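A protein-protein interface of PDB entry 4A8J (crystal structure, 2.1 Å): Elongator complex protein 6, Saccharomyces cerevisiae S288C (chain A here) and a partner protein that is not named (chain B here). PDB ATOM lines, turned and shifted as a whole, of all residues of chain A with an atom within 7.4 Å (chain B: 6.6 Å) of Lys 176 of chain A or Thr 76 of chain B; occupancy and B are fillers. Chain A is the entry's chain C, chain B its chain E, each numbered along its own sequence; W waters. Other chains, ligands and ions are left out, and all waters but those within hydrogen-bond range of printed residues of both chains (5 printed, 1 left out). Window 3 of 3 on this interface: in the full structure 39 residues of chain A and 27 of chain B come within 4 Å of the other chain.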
ATOM      1  N   ARG A 129       5.424  26.113  18.428  1.00  0.00           N
ATOM      2  CA  ARG A 129       4.142  26.284  19.095  1.00  0.00           C
ATOM      3  C   ARG A 129       3.289  25.007  19.093  1.00  0.00           C
ATOM      4  O   ARG A 129       2.847  24.528  20.152  1.00  0.00           O
ATOM      5  CB  ARG A 129       3.392  27.434  18.427  1.00  0.00           C
ATOM      6  CG  ARG A 129       2.751  28.402  19.389  1.00  0.00           C
ATOM      7  CD  ARG A 129       2.698  29.790  18.790  1.00  0.00           C
ATOM      8  NE  ARG A 129       2.407  29.737  17.362  1.00  0.00           N
ATOM      9  CZ  ARG A 129       3.191  30.244  16.417  1.00  0.00           C
ATOM     10  NH1 ARG A 129       4.321  30.869  16.739  1.00  0.00           N
ATOM     11  NH2 ARG A 129       2.834  30.133  15.146  1.00  0.00           N
ATOM     12  N   ASP A 130       3.075  24.452  17.900  1.00  0.00           N
ATOM     13  CA  ASP A 130       2.207  23.281  17.733  1.00  0.00           C
ATOM     14  C   ASP A 130       2.625  22.088  18.574  1.00  0.00           C
ATOM     15  O   ASP A 130       1.778  21.391  19.161  1.00  0.00           O
ATOM     16  CB  ASP A 130       2.138  22.862  16.264  1.00  0.00           C
ATOM     17  CG  ASP A 130       1.214  23.753  15.449  1.00  0.00           C
ATOM     18  OD1 ASP A 130       0.178  24.191  16.001  1.00  0.00           O
ATOM     19  OD2 ASP A 130       1.523  24.013  14.262  1.00  0.00           O
ATOM     20  N   LEU A 133       1.982  22.802  22.445  1.00  0.00           N
ATOM     21  CA  LEU A 133       0.583  22.605  22.821  1.00  0.00           C
ATOM     22  C   LEU A 133       0.202  21.132  22.775  1.00  0.00           C
ATOM     23  O   LEU A 133      -0.457  20.614  23.691  1.00  0.00           O
ATOM     24  CB  LEU A 133      -0.336  23.428  21.919  1.00  0.00           C
ATOM     25  CG  LEU A 133      -0.192  24.947  22.067  1.00  0.00           C
ATOM     26  CD1 LEU A 133      -1.239  25.678  21.249  1.00  0.00           C
ATOM     27  CD2 LEU A 133      -0.274  25.347  23.537  1.00  0.00           C
ATOM     28  N   SER A 134       0.617  20.448  21.711  1.00  0.00           N
ATOM     29  CA  SER A 134       0.315  19.027  21.583  1.00  0.00           C
ATOM     30  C   SER A 134       0.890  18.211  22.754  1.00  0.00           C
ATOM     31  O   SER A 134       0.227  17.307  23.266  1.00  0.00           O
ATOM     32  CB  SER A 134       0.798  18.480  20.230  1.00  0.00           C
ATOM     33  OG  SER A 134       2.167  18.132  20.290  1.00  0.00           O
ATOM     34  N   ASP A 135       2.110  18.530  23.190  1.00  0.00           N
ATOM     35  CA  ASP A 135       2.703  17.835  24.341  1.00  0.00           C
ATOM     36  C   ASP A 135       1.925  18.075  25.639  1.00  0.00           C
ATOM     37  O   ASP A 135       1.658  17.129  26.423  1.00  0.00           O
ATOM     38  CB  ASP A 135       4.178  18.233  24.533  1.00  0.00           C
ATOM     39  CG  ASP A 135       5.123  17.444  23.635  1.00  0.00           C
ATOM     40  OD1 ASP A 135       4.659  16.500  22.952  1.00  0.00           O
ATOM     41  OD2 ASP A 135       6.332  17.761  23.621  1.00  0.00           O
ATOM     42  N   VAL A 136       1.557  19.340  25.876  1.00  0.00           N
ATOM     43  CA  VAL A 136       0.738  19.617  27.068  1.00  0.00           C
ATOM     44  C   VAL A 136      -0.577  18.789  27.067  1.00  0.00           C
ATOM     45  O   VAL A 136      -0.955  18.101  28.053  1.00  0.00           O
ATOM     46  CB  VAL A 136       0.422  21.115  27.175  1.00  0.00           C
ATOM     47  CG1 VAL A 136      -0.591  21.368  28.291  1.00  0.00           C
ATOM     48  CG2 VAL A 136       1.694  21.871  27.429  1.00  0.00           C
ATOM     49  N   LEU A 137      -1.268  18.858  25.935  1.00  0.00           N
ATOM     50  CA  LEU A 137      -2.519  18.138  25.786  1.00  0.00           C
ATOM     51  C   LEU A 137      -2.297  16.660  26.050  1.00  0.00           C
ATOM     52  O   LEU A 137      -3.087  16.028  26.747  1.00  0.00           O
ATOM     53  CB  LEU A 137      -3.092  18.328  24.390  1.00  0.00           C
ATOM     54  CG  LEU A 137      -4.420  17.608  24.103  1.00  0.00           C
ATOM     55  CD1 LEU A 137      -5.453  17.927  25.184  1.00  0.00           C
ATOM     56  CD2 LEU A 137      -4.948  18.001  22.717  1.00  0.00           C
ATOM     57  N   LEU A 168       1.919  33.033  20.236  1.00  0.00           N
ATOM     58  CA  LEU A 168       0.708  32.237  20.485  1.00  0.00           C
ATOM     59  C   LEU A 168      -0.541  33.128  20.610  1.00  0.00           C
ATOM     60  O   LEU A 168      -0.601  34.023  21.469  1.00  0.00           O
ATOM     61  CB  LEU A 168       0.881  31.406  21.758  1.00  0.00           C
ATOM     62  CG  LEU A 168      -0.267  30.443  22.072  1.00  0.00           C
ATOM     63  CD1 LEU A 168      -0.489  29.493  20.896  1.00  0.00           C
ATOM     64  CD2 LEU A 168       0.003  29.675  23.349  1.00  0.00           C
ATOM     65  N   CYS A 170      -4.731  33.684  21.215  1.00  0.00           N
ATOM     66  CA  CYS A 170      -5.848  33.110  21.925  1.00  0.00           C
ATOM     67  C   CYS A 170      -6.549  32.014  21.099  1.00  0.00           C
ATOM     68  O   CYS A 170      -6.889  30.946  21.615  1.00  0.00           O
ATOM     69  CB  CYS A 170      -6.848  34.209  22.282  1.00  0.00           C
ATOM     70  SG  CYS A 170      -8.168  33.591  23.358  1.00  0.00           S
ATOM     71  N   SER A 171      -6.784  32.268  19.819  1.00  0.00           N
ATOM     72  CA  SER A 171      -7.519  31.274  19.047  1.00  0.00           C
ATOM     73  C   SER A 171      -6.736  29.966  18.863  1.00  0.00           C
ATOM     74  O   SER A 171      -7.320  28.882  18.839  1.00  0.00           O
ATOM     75  CB  SER A 171      -7.993  31.851  17.710  1.00  0.00           C
ATOM     76  OG  SER A 171      -6.891  32.135  16.880  1.00  0.00           O
ATOM     77  N   GLU A 172      -5.417  30.051  18.744  1.00  0.00           N
ATOM     78  CA  GLU A 172      -4.615  28.836  18.662  1.00  0.00           C
ATOM     79  C   GLU A 172      -4.621  28.108  20.000  1.00  0.00           C
ATOM     80  O   GLU A 172      -4.728  26.878  20.054  1.00  0.00           O
ATOM     81  CB  GLU A 172      -3.174  29.140  18.222  1.00  0.00           C
ATOM     82  CG  GLU A 172      -2.329  27.875  18.046  1.00  0.00           C
ATOM     83  CD  GLU A 172      -1.025  28.111  17.268  1.00  0.00           C
ATOM     84  OE1 GLU A 172      -0.610  29.282  17.112  1.00  0.00           O
ATOM     85  OE2 GLU A 172      -0.411  27.121  16.808  1.00  0.00           O
ATOM     86  N   LEU A 173      -4.487  28.859  21.089  1.00  0.00           N
ATOM     87  CA  LEU A 173      -4.548  28.233  22.409  1.00  0.00           C
ATOM     88  C   LEU A 173      -5.866  27.481  22.590  1.00  0.00           C
ATOM     89  O   LEU A 173      -5.880  26.357  23.080  1.00  0.00           O
ATOM     90  CB  LEU A 173      -4.324  29.266  23.538  1.00  0.00           C
ATOM     91  CG  LEU A 173      -4.428  28.759  24.990  1.00  0.00           C
ATOM     92  CD1 LEU A 173      -3.370  27.686  25.313  1.00  0.00           C
ATOM     93  CD2 LEU A 173      -4.291  29.945  25.954  1.00  0.00           C
ATOM     94  N   ASN A 174      -6.972  28.084  22.173  1.00  0.00           N
ATOM     95  CA  ASN A 174      -8.270  27.410  22.304  1.00  0.00           C
ATOM     96  C   ASN A 174      -8.420  26.217  21.356  1.00  0.00           C
ATOM     97  O   ASN A 174      -8.774  25.120  21.785  1.00  0.00           O
ATOM     98  CB  ASN A 174      -9.431  28.407  22.118  1.00  0.00           C
ATOM     99  CG  ASN A 174      -9.658  29.276  23.355  1.00  0.00           C
ATOM    100  OD1 ASN A 174      -9.312  28.881  24.469  1.00  0.00           O
ATOM    101  ND2 ASN A 174     -10.246  30.456  23.162  1.00  0.00           N
ATOM    102  N   ASN A 175      -8.114  26.431  20.081  1.00  0.00           N
ATOM    103  CA  ASN A 175      -8.256  25.395  19.065  1.00  0.00           C
ATOM    104  C   ASN A 175      -7.390  24.169  19.288  1.00  0.00           C
ATOM    105  O   ASN A 175      -7.816  23.052  18.998  1.00  0.00           O
ATOM    106  CB  ASN A 175      -7.960  25.951  17.664  1.00  0.00           C
ATOM    107  CG  ASN A 175      -9.011  26.921  17.198  1.00  0.00           C
ATOM    108  OD1 ASN A 175     -10.125  26.952  17.735  1.00  0.00           O
ATOM    109  ND2 ASN A 175      -8.661  27.744  16.199  1.00  0.00           N
ATOM    110  N   LYS A 176      -6.181  24.378  19.799  1.00  0.00           N
ATOM    111  CA  LYS A 176      -5.188  23.303  19.874  1.00  0.00           C
ATOM    112  C   LYS A 176      -4.991  22.740  21.271  1.00  0.00           C
ATOM    113  O   LYS A 176      -4.291  21.747  21.442  1.00  0.00           O
ATOM    114  CB  LYS A 176      -3.825  23.804  19.370  1.00  0.00           C
ATOM    115  CG  LYS A 176      -3.792  24.228  17.920  1.00  0.00           C
ATOM    116  CD  LYS A 176      -3.957  23.029  17.003  1.00  0.00           C
ATOM    117  CE  LYS A 176      -4.734  23.421  15.751  1.00  0.00           C
ATOM    118  NZ  LYS A 176      -4.324  24.770  15.275  1.00  0.00           N
ATOM    119  N   PHE A 177      -5.567  23.380  22.282  1.00  0.00           N
ATOM    120  CA  PHE A 177      -5.418  22.866  23.653  1.00  0.00           C
ATOM    121  C   PHE A 177      -6.726  22.863  24.449  1.00  0.00           C
ATOM    122  O   PHE A 177      -7.235  21.809  24.837  1.00  0.00           O
ATOM    123  CB  PHE A 177      -4.321  23.646  24.389  1.00  0.00           C
ATOM    124  CG  PHE A 177      -4.167  23.284  25.862  1.00  0.00           C
ATOM    125  CD1 PHE A 177      -4.129  21.977  26.272  1.00  0.00           C
ATOM    126  CD2 PHE A 177      -4.007  24.280  26.821  1.00  0.00           C
ATOM    127  CE1 PHE A 177      -3.975  21.652  27.620  1.00  0.00           C
ATOM    128  CE2 PHE A 177      -3.845  23.966  28.175  1.00  0.00           C
ATOM    129  CZ  PHE A 177      -3.826  22.654  28.568  1.00  0.00           C
ATOM    130  N   ILE A 178      -7.266  24.045  24.703  1.00  0.00           N
ATOM    131  CA  ILE A 178      -8.389  24.164  25.624  1.00  0.00           C
ATOM    132  C   ILE A 178      -9.601  23.362  25.139  1.00  0.00           C
ATOM    133  O   ILE A 178     -10.125  22.511  25.856  1.00  0.00           O
ATOM    134  CB  ILE A 178      -8.762  25.652  25.859  1.00  0.00           C
ATOM    135  CG1 ILE A 178      -7.622  26.374  26.581  1.00  0.00           C
ATOM    136  CG2 ILE A 178     -10.044  25.774  26.660  1.00  0.00           C
ATOM    137  CD1 ILE A 178      -7.201  25.707  27.903  1.00  0.00           C
ATOM    138  N   THR A 179     -10.021  23.619  23.904  1.00  0.00           N
ATOM    139  CA  THR A 179     -11.215  22.989  23.345  1.00  0.00           C
ATOM    140  C   THR A 179     -11.124  21.458  23.222  1.00  0.00           C
ATOM    141  O   THR A 179     -12.046  20.759  23.632  1.00  0.00           O
ATOM    142  CB  THR A 179     -11.628  23.650  22.012  1.00  0.00           C
ATOM    143  OG1 THR A 179     -11.966  25.028  22.259  1.00  0.00           O
ATOM    144  CG2 THR A 179     -12.838  22.945  21.416  1.00  0.00           C
ATOM    145  N   PRO A 180     -10.001  20.932  22.694  1.00  0.00           N
ATOM    146  CA  PRO A 180      -9.770  19.476  22.725  1.00  0.00           C
ATOM    147  C   PRO A 180      -9.799  18.928  24.158  1.00  0.00           C
ATOM    148  O   PRO A 180     -10.377  17.856  24.431  1.00  0.00           O
ATOM    149  CB  PRO A 180      -8.350  19.335  22.149  1.00  0.00           C
ATOM    150  CG  PRO A 180      -8.141  20.544  21.340  1.00  0.00           C
ATOM    151  CD  PRO A 180      -8.939  21.646  21.967  1.00  0.00           C
ATOM    152  N   LEU A 181      -9.182  19.665  25.079  1.00  0.00           N
ATOM    153  CA  LEU A 181      -9.163  19.229  26.474  1.00  0.00           C
ATOM    154  C   LEU A 181     -10.596  19.064  26.957  1.00  0.00           C
ATOM    155  O   LEU A 181     -10.984  17.994  27.448  1.00  0.00           O
ATOM    156  CB  LEU A 181      -8.382  20.217  27.359  1.00  0.00           C
ATOM    157  CG  LEU A 181      -8.396  19.952  28.876  1.00  0.00           C
ATOM    158  CD1 LEU A 181      -8.011  18.507  29.178  1.00  0.00           C
ATOM    159  CD2 LEU A 181      -7.464  20.931  29.630  1.00  0.00           C
ATOM    160  N   ARG A 183     -13.292  18.731  25.320  1.00  0.00           N
ATOM    161  CA  ARG A 183     -13.962  17.682  24.559  1.00  0.00           C
ATOM    162  C   ARG A 183     -13.646  16.301  25.149  1.00  0.00           C
ATOM    163  O   ARG A 183     -14.370  15.333  24.897  1.00  0.00           O
ATOM    164  CB  ARG A 183     -13.551  17.766  23.071  1.00  0.00           C
ATOM    165  CG  ARG A 183     -14.627  17.364  22.086  1.00  0.00           C
ATOM    166  CD  ARG A 183     -14.155  17.464  20.634  1.00  0.00           C
ATOM    167  NE  ARG A 183     -13.932  18.846  20.240  1.00  0.00           N
ATOM    168  CZ  ARG A 183     -14.833  19.617  19.642  1.00  0.00           C
ATOM    169  NH1 ARG A 183     -16.036  19.145  19.340  1.00  0.00           N
ATOM    170  NH2 ARG A 183     -14.521  20.865  19.338  1.00  0.00           N
ATOM    171  N   SER B  59     -18.628  24.155  14.188  1.00  0.00           N
ATOM    172  CA  SER B  59     -18.223  24.409  15.569  1.00  0.00           C
ATOM    173  C   SER B  59     -16.758  24.761  15.704  1.00  0.00           C
ATOM    174  O   SER B  59     -15.893  23.895  15.533  1.00  0.00           O
ATOM    175  CB  SER B  59     -18.499  23.176  16.433  1.00  0.00           C
ATOM    176  OG  SER B  59     -17.982  23.350  17.739  1.00  0.00           O
ATOM    177  N   PHE B  60     -16.488  26.032  15.994  1.00  0.00           N
ATOM    178  CA  PHE B  60     -15.162  26.449  16.440  1.00  0.00           C
ATOM    179  C   PHE B  60     -15.061  26.381  17.952  1.00  0.00           C
ATOM    180  O   PHE B  60     -13.973  26.238  18.496  1.00  0.00           O
ATOM    181  CB  PHE B  60     -14.831  27.868  15.979  1.00  0.00           C
ATOM    182  CG  PHE B  60     -14.548  27.971  14.512  1.00  0.00           C
ATOM    183  CD1 PHE B  60     -13.299  27.628  14.009  1.00  0.00           C
ATOM    184  CD2 PHE B  60     -15.533  28.388  13.634  1.00  0.00           C
ATOM    185  CE1 PHE B  60     -13.041  27.730  12.641  1.00  0.00           C
ATOM    186  CE2 PHE B  60     -15.285  28.478  12.269  1.00  0.00           C
ATOM    187  CZ  PHE B  60     -14.038  28.150  11.776  1.00  0.00           C
ATOM    188  N   GLU B  61     -16.187  26.506  18.642  1.00  0.00           N
ATOM    189  CA  GLU B  61     -16.118  26.582  20.099  1.00  0.00           C
ATOM    190  C   GLU B  61     -17.255  25.857  20.830  1.00  0.00           C
ATOM    191  O   GLU B  61     -17.495  26.102  22.003  1.00  0.00           O
ATOM    192  CB  GLU B  61     -16.032  28.045  20.542  1.00  0.00           C
ATOM    193  CG  GLU B  61     -17.280  28.823  20.242  1.00  0.00           C
ATOM    194  CD  GLU B  61     -17.130  30.312  20.504  1.00  0.00           C
ATOM    195  OE1 GLU B  61     -15.984  30.802  20.656  1.00  0.00           O
ATOM    196  OE2 GLU B  61     -18.175  30.994  20.560  1.00  0.00           O
ATOM    197  N   THR B  62     -17.940  24.944  20.147  1.00  0.00           N
ATOM    198  CA  THR B  62     -19.020  24.183  20.776  1.00  0.00           C
ATOM    199  C   THR B  62     -18.642  22.711  20.914  1.00  0.00           C
ATOM    200  O   THR B  62     -18.519  22.005  19.908  1.00  0.00           O
ATOM    201  CB  THR B  62     -20.316  24.246  19.934  1.00  0.00           C
ATOM    202  OG1 THR B  62     -20.651  25.608  19.639  1.00  0.00           O
ATOM    203  CG2 THR B  62     -21.468  23.600  20.681  1.00  0.00           C
ATOM    204  N   ILE B  73     -19.731  19.604  12.415  1.00  0.00           N
ATOM    205  CA  ILE B  73     -18.374  19.715  11.926  1.00  0.00           C
ATOM    206  C   ILE B  73     -17.514  20.425  12.970  1.00  0.00           C
ATOM    207  O   ILE B  73     -17.819  21.549  13.362  1.00  0.00           O
ATOM    208  CB  ILE B  73     -18.332  20.525  10.610  1.00  0.00           C
ATOM    209  CG1 ILE B  73     -19.181  19.853   9.525  1.00  0.00           C
ATOM    210  CG2 ILE B  73     -16.913  20.667  10.124  1.00  0.00           C
ATOM    211  CD1 ILE B  73     -19.361  20.706   8.286  1.00  0.00           C
ATOM    212  N   ASP B  74     -16.443  19.769  13.406  1.00  0.00           N
ATOM    213  CA  ASP B  74     -15.470  20.366  14.320  1.00  0.00           C
ATOM    214  C   ASP B  74     -14.419  21.106  13.522  1.00  0.00           C
ATOM    215  O   ASP B  74     -13.521  20.493  12.950  1.00  0.00           O
ATOM    216  CB  ASP B  74     -14.821  19.271  15.175  1.00  0.00           C
ATOM    217  CG  ASP B  74     -13.632  19.775  15.990  1.00  0.00           C
ATOM    218  OD1 ASP B  74     -13.528  20.999  16.260  1.00  0.00           O
ATOM    219  OD2 ASP B  74     -12.801  18.926  16.369  1.00  0.00           O
ATOM    220  N   ALA B  75     -14.525  22.431  13.480  1.00  0.00           N
ATOM    221  CA  ALA B  75     -13.649  23.235  12.619  1.00  0.00           C
ATOM    222  C   ALA B  75     -12.290  23.524  13.231  1.00  0.00           C
ATOM    223  O   ALA B  75     -11.428  24.117  12.583  1.00  0.00           O
ATOM    224  CB  ALA B  75     -14.330  24.541  12.210  1.00  0.00           C
ATOM    225  N   THR B  76     -12.088  23.105  14.476  1.00  0.00           N
ATOM    226  CA  THR B  76     -10.912  23.556  15.220  1.00  0.00           C
ATOM    227  C   THR B  76      -9.579  22.918  14.815  1.00  0.00           C
ATOM    228  O   THR B  76      -8.520  23.442  15.155  1.00  0.00           O
ATOM    229  CB  THR B  76     -11.109  23.395  16.728  1.00  0.00           C
ATOM    230  OG1 THR B  76     -11.232  22.000  17.051  1.00  0.00           O
ATOM    231  CG2 THR B  76     -12.352  24.165  17.186  1.00  0.00           C
ATOM    232  N   GLN B  77      -9.616  21.798  14.107  1.00  0.00           N
ATOM    233  CA  GLN B  77      -8.376  21.096  13.800  1.00  0.00           C
ATOM    234  C   GLN B  77      -7.964  21.230  12.332  1.00  0.00           C
ATOM    235  O   GLN B  77      -6.778  21.154  12.001  1.00  0.00           O
ATOM    236  CB  GLN B  77      -8.487  19.622  14.203  1.00  0.00           C
ATOM    237  CG  GLN B  77      -8.871  19.401  15.668  1.00  0.00           C
ATOM    238  CD  GLN B  77      -7.858  19.990  16.646  1.00  0.00           C
ATOM    239  OE1 GLN B  77      -6.651  19.789  16.506  1.00  0.00           O
ATOM    240  NE2 GLN B  77      -8.349  20.728  17.636  1.00  0.00           N
ATOM    241  N   MET B  78      -8.947  21.443  11.462  1.00  0.00           N
ATOM    242  CA  MET B  78      -8.716  21.464  10.017  1.00  0.00           C
ATOM    243  C   MET B  78      -8.651  22.884   9.443  1.00  0.00           C
ATOM    244  O   MET B  78      -9.220  23.819  10.010  1.00  0.00           O
ATOM    245  CB  MET B  78      -9.793  20.652   9.290  1.00  0.00           C
ATOM    246  CG  MET B  78     -11.212  21.181   9.477  1.00  0.00           C
ATOM    247  SD  MET B  78     -12.589  20.274   8.373  1.00  0.00           S
ATOM    248  CE  MET B  78     -14.168  21.086   9.115  1.00  0.00           C
ATOM    249  N   TYR B 111     -13.429  33.366  14.333  1.00  0.00           N
ATOM    250  CA  TYR B 111     -12.306  32.464  14.105  1.00  0.00           C
ATOM    251  C   TYR B 111     -11.825  32.468  12.658  1.00  0.00           C
ATOM    252  O   TYR B 111     -10.809  31.849  12.342  1.00  0.00           O
ATOM    253  CB  TYR B 111     -12.672  31.038  14.550  1.00  0.00           C
ATOM    254  CG  TYR B 111     -12.740  30.870  16.062  1.00  0.00           C
ATOM    255  CD1 TYR B 111     -13.903  31.178  16.766  1.00  0.00           C
ATOM    256  CD2 TYR B 111     -11.638  30.410  16.786  1.00  0.00           C
ATOM    257  CE1 TYR B 111     -13.970  31.033  18.157  1.00  0.00           C
ATOM    258  CE2 TYR B 111     -11.694  30.261  18.177  1.00  0.00           C
ATOM    259  CZ  TYR B 111     -12.861  30.579  18.854  1.00  0.00           C
ATOM    260  OH  TYR B 111     -12.922  30.435  20.232  1.00  0.00           O
HETATM  261  O   HOH W   1      -9.133  29.634  13.682  1.00  0.00           O
HETATM  262  O   HOH W   2     -11.637  26.673  19.954  1.00  0.00           O
HETATM  263  O   HOH W   3     -10.743  31.711  20.710  1.00  0.00           O
HETATM  264  O   HOH W   4     -11.223  19.132  19.158  1.00  0.00           O
HETATM  265  O   HOH W   5     -12.718  28.671  21.852  1.00  0.00           O
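The side-chain carboxylate (OD1) of Asp 74 of chain B lies within salt-bridge range of the guanidinium group (NH2) of Arg 183 of chain A, 3.2 Å away.
The side-chain amide nitrogen (NE2) of Gln 77 of chain B is in hydrogen-bond range of the backbone carbonyl oxygen (O) of Asn 175 of chain A, at 2.7 Å.
OG of Ser 59 of chain B sits at hydrogen-bond distance from O of Thr 62 of chain B, 2.6 Å away.
The side-chain hydroxyl (OH) of Tyr 111 of chain B is in hydrogen-bond range of the side-chain carboxylate (OE1) of Glu 61 of chain B (3.1 Å).
The side-chain hydroxyl (OG1) of Thr 76 of chain B sits at hydrogen-bond distance from the side-chain amide nitrogen (NE2) of Gln 77 of chain B.
The side-chain sulfur of Cys 170 of chain A is in hydrogen-bond range of the side-chain amide nitrogen of Asn 174 of chain A, 3.8 Å away.
O of Ser 171 of chain A sits close to ND2 of Asn 175 of chain A (3.2 Å).
The backbone NH (N) of Thr 179 of chain A sits at hydrogen-bond distance from the backbone carbonyl oxygen (O) of Asn 174 of chain A.
Among the printed residues, merely in contact across the chains: Asn 174 of chain A with Tyr 111 of chain B, Asn 175 of chain A with Phe 60 of chain B, Asn 175 of chain A with Thr 76 of chain B, Asn 175 of chain A with Tyr 111 of chain B, Lys 176 of chain A with Thr 76 of chain B, Pro 180 of chain A with Gln 77 of chain B and Arg 183 of chain A with Thr 62 of chain B.
Lys 176 of chain A touches just one residue of chain B: Thr 76 (3.8 Å).
Thr 76 of chain B touches just these residues of chain A: Asn 175 (3.6 Å) and Lys 176 (3.8 Å).
Printed residues of chain B within 4 Å of Pro 180 of chain A: Gln 77.
Printed residues of chain A within 4 Å of Asp 74 of chain B: Arg 183.
Ala 75 of chain B touches none of the printed residues of chain A.
The nearest residue of chain A that does not touch Thr 76 of chain B is Arg 183 of chain A (4.2 Å).
The nearest printed residue of chain B that does not touch Asn 174 of chain A is Thr 76 of chain B (5.8 Å).
Printed residues of chain B that touch a printed residue of chain A: Phe 60, Thr 62, Asp 74, Thr 76, Gln 77 and Tyr 111.
Of the 21 printed residues of chain A, 5 touch a printed residue of chain B.
Hydrophobic or aromatic side chains of chain A within 4 Å of the printed part of chain B: Pro 180.
Among the printed residues, Asp or Glu carboxylates within 4 Å of a Lys or Arg side-chain nitrogen of the other chain: Arg 183 of chain A with Asp 74 of chain B.
Water W5 lies within hydrogen-bond range of the side-chain hydroxyl (OH) of Tyr 111 of chain B (2.4 Å) and the side-chain amide nitrogen (ND2) of Asn 174 of chain A (3.3 Å).
Water W3 lies within hydrogen-bond range of OH of Tyr 111 of chain B and ND2 of Asn 174 of chain A.
Water W2 lies within hydrogen-bond range of OD1 of Asn 175 of chain A (2.7 Å), O of Phe 60 of chain B (2.8 Å) and OG1 of Thr 179 of chain A (2.9 Å).
Water W4 bridges NE of Arg 183 of chain A (2.9 Å) and OD2 of Asp 74 of chain B (3.2 Å).
Water W1 bridges the backbone carbonyl oxygen (O) of Tyr 111 of chain B (3.1 Å) and the side-chain amide nitrogen (ND2) of Asn 175 of chain A (3.2 Å).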
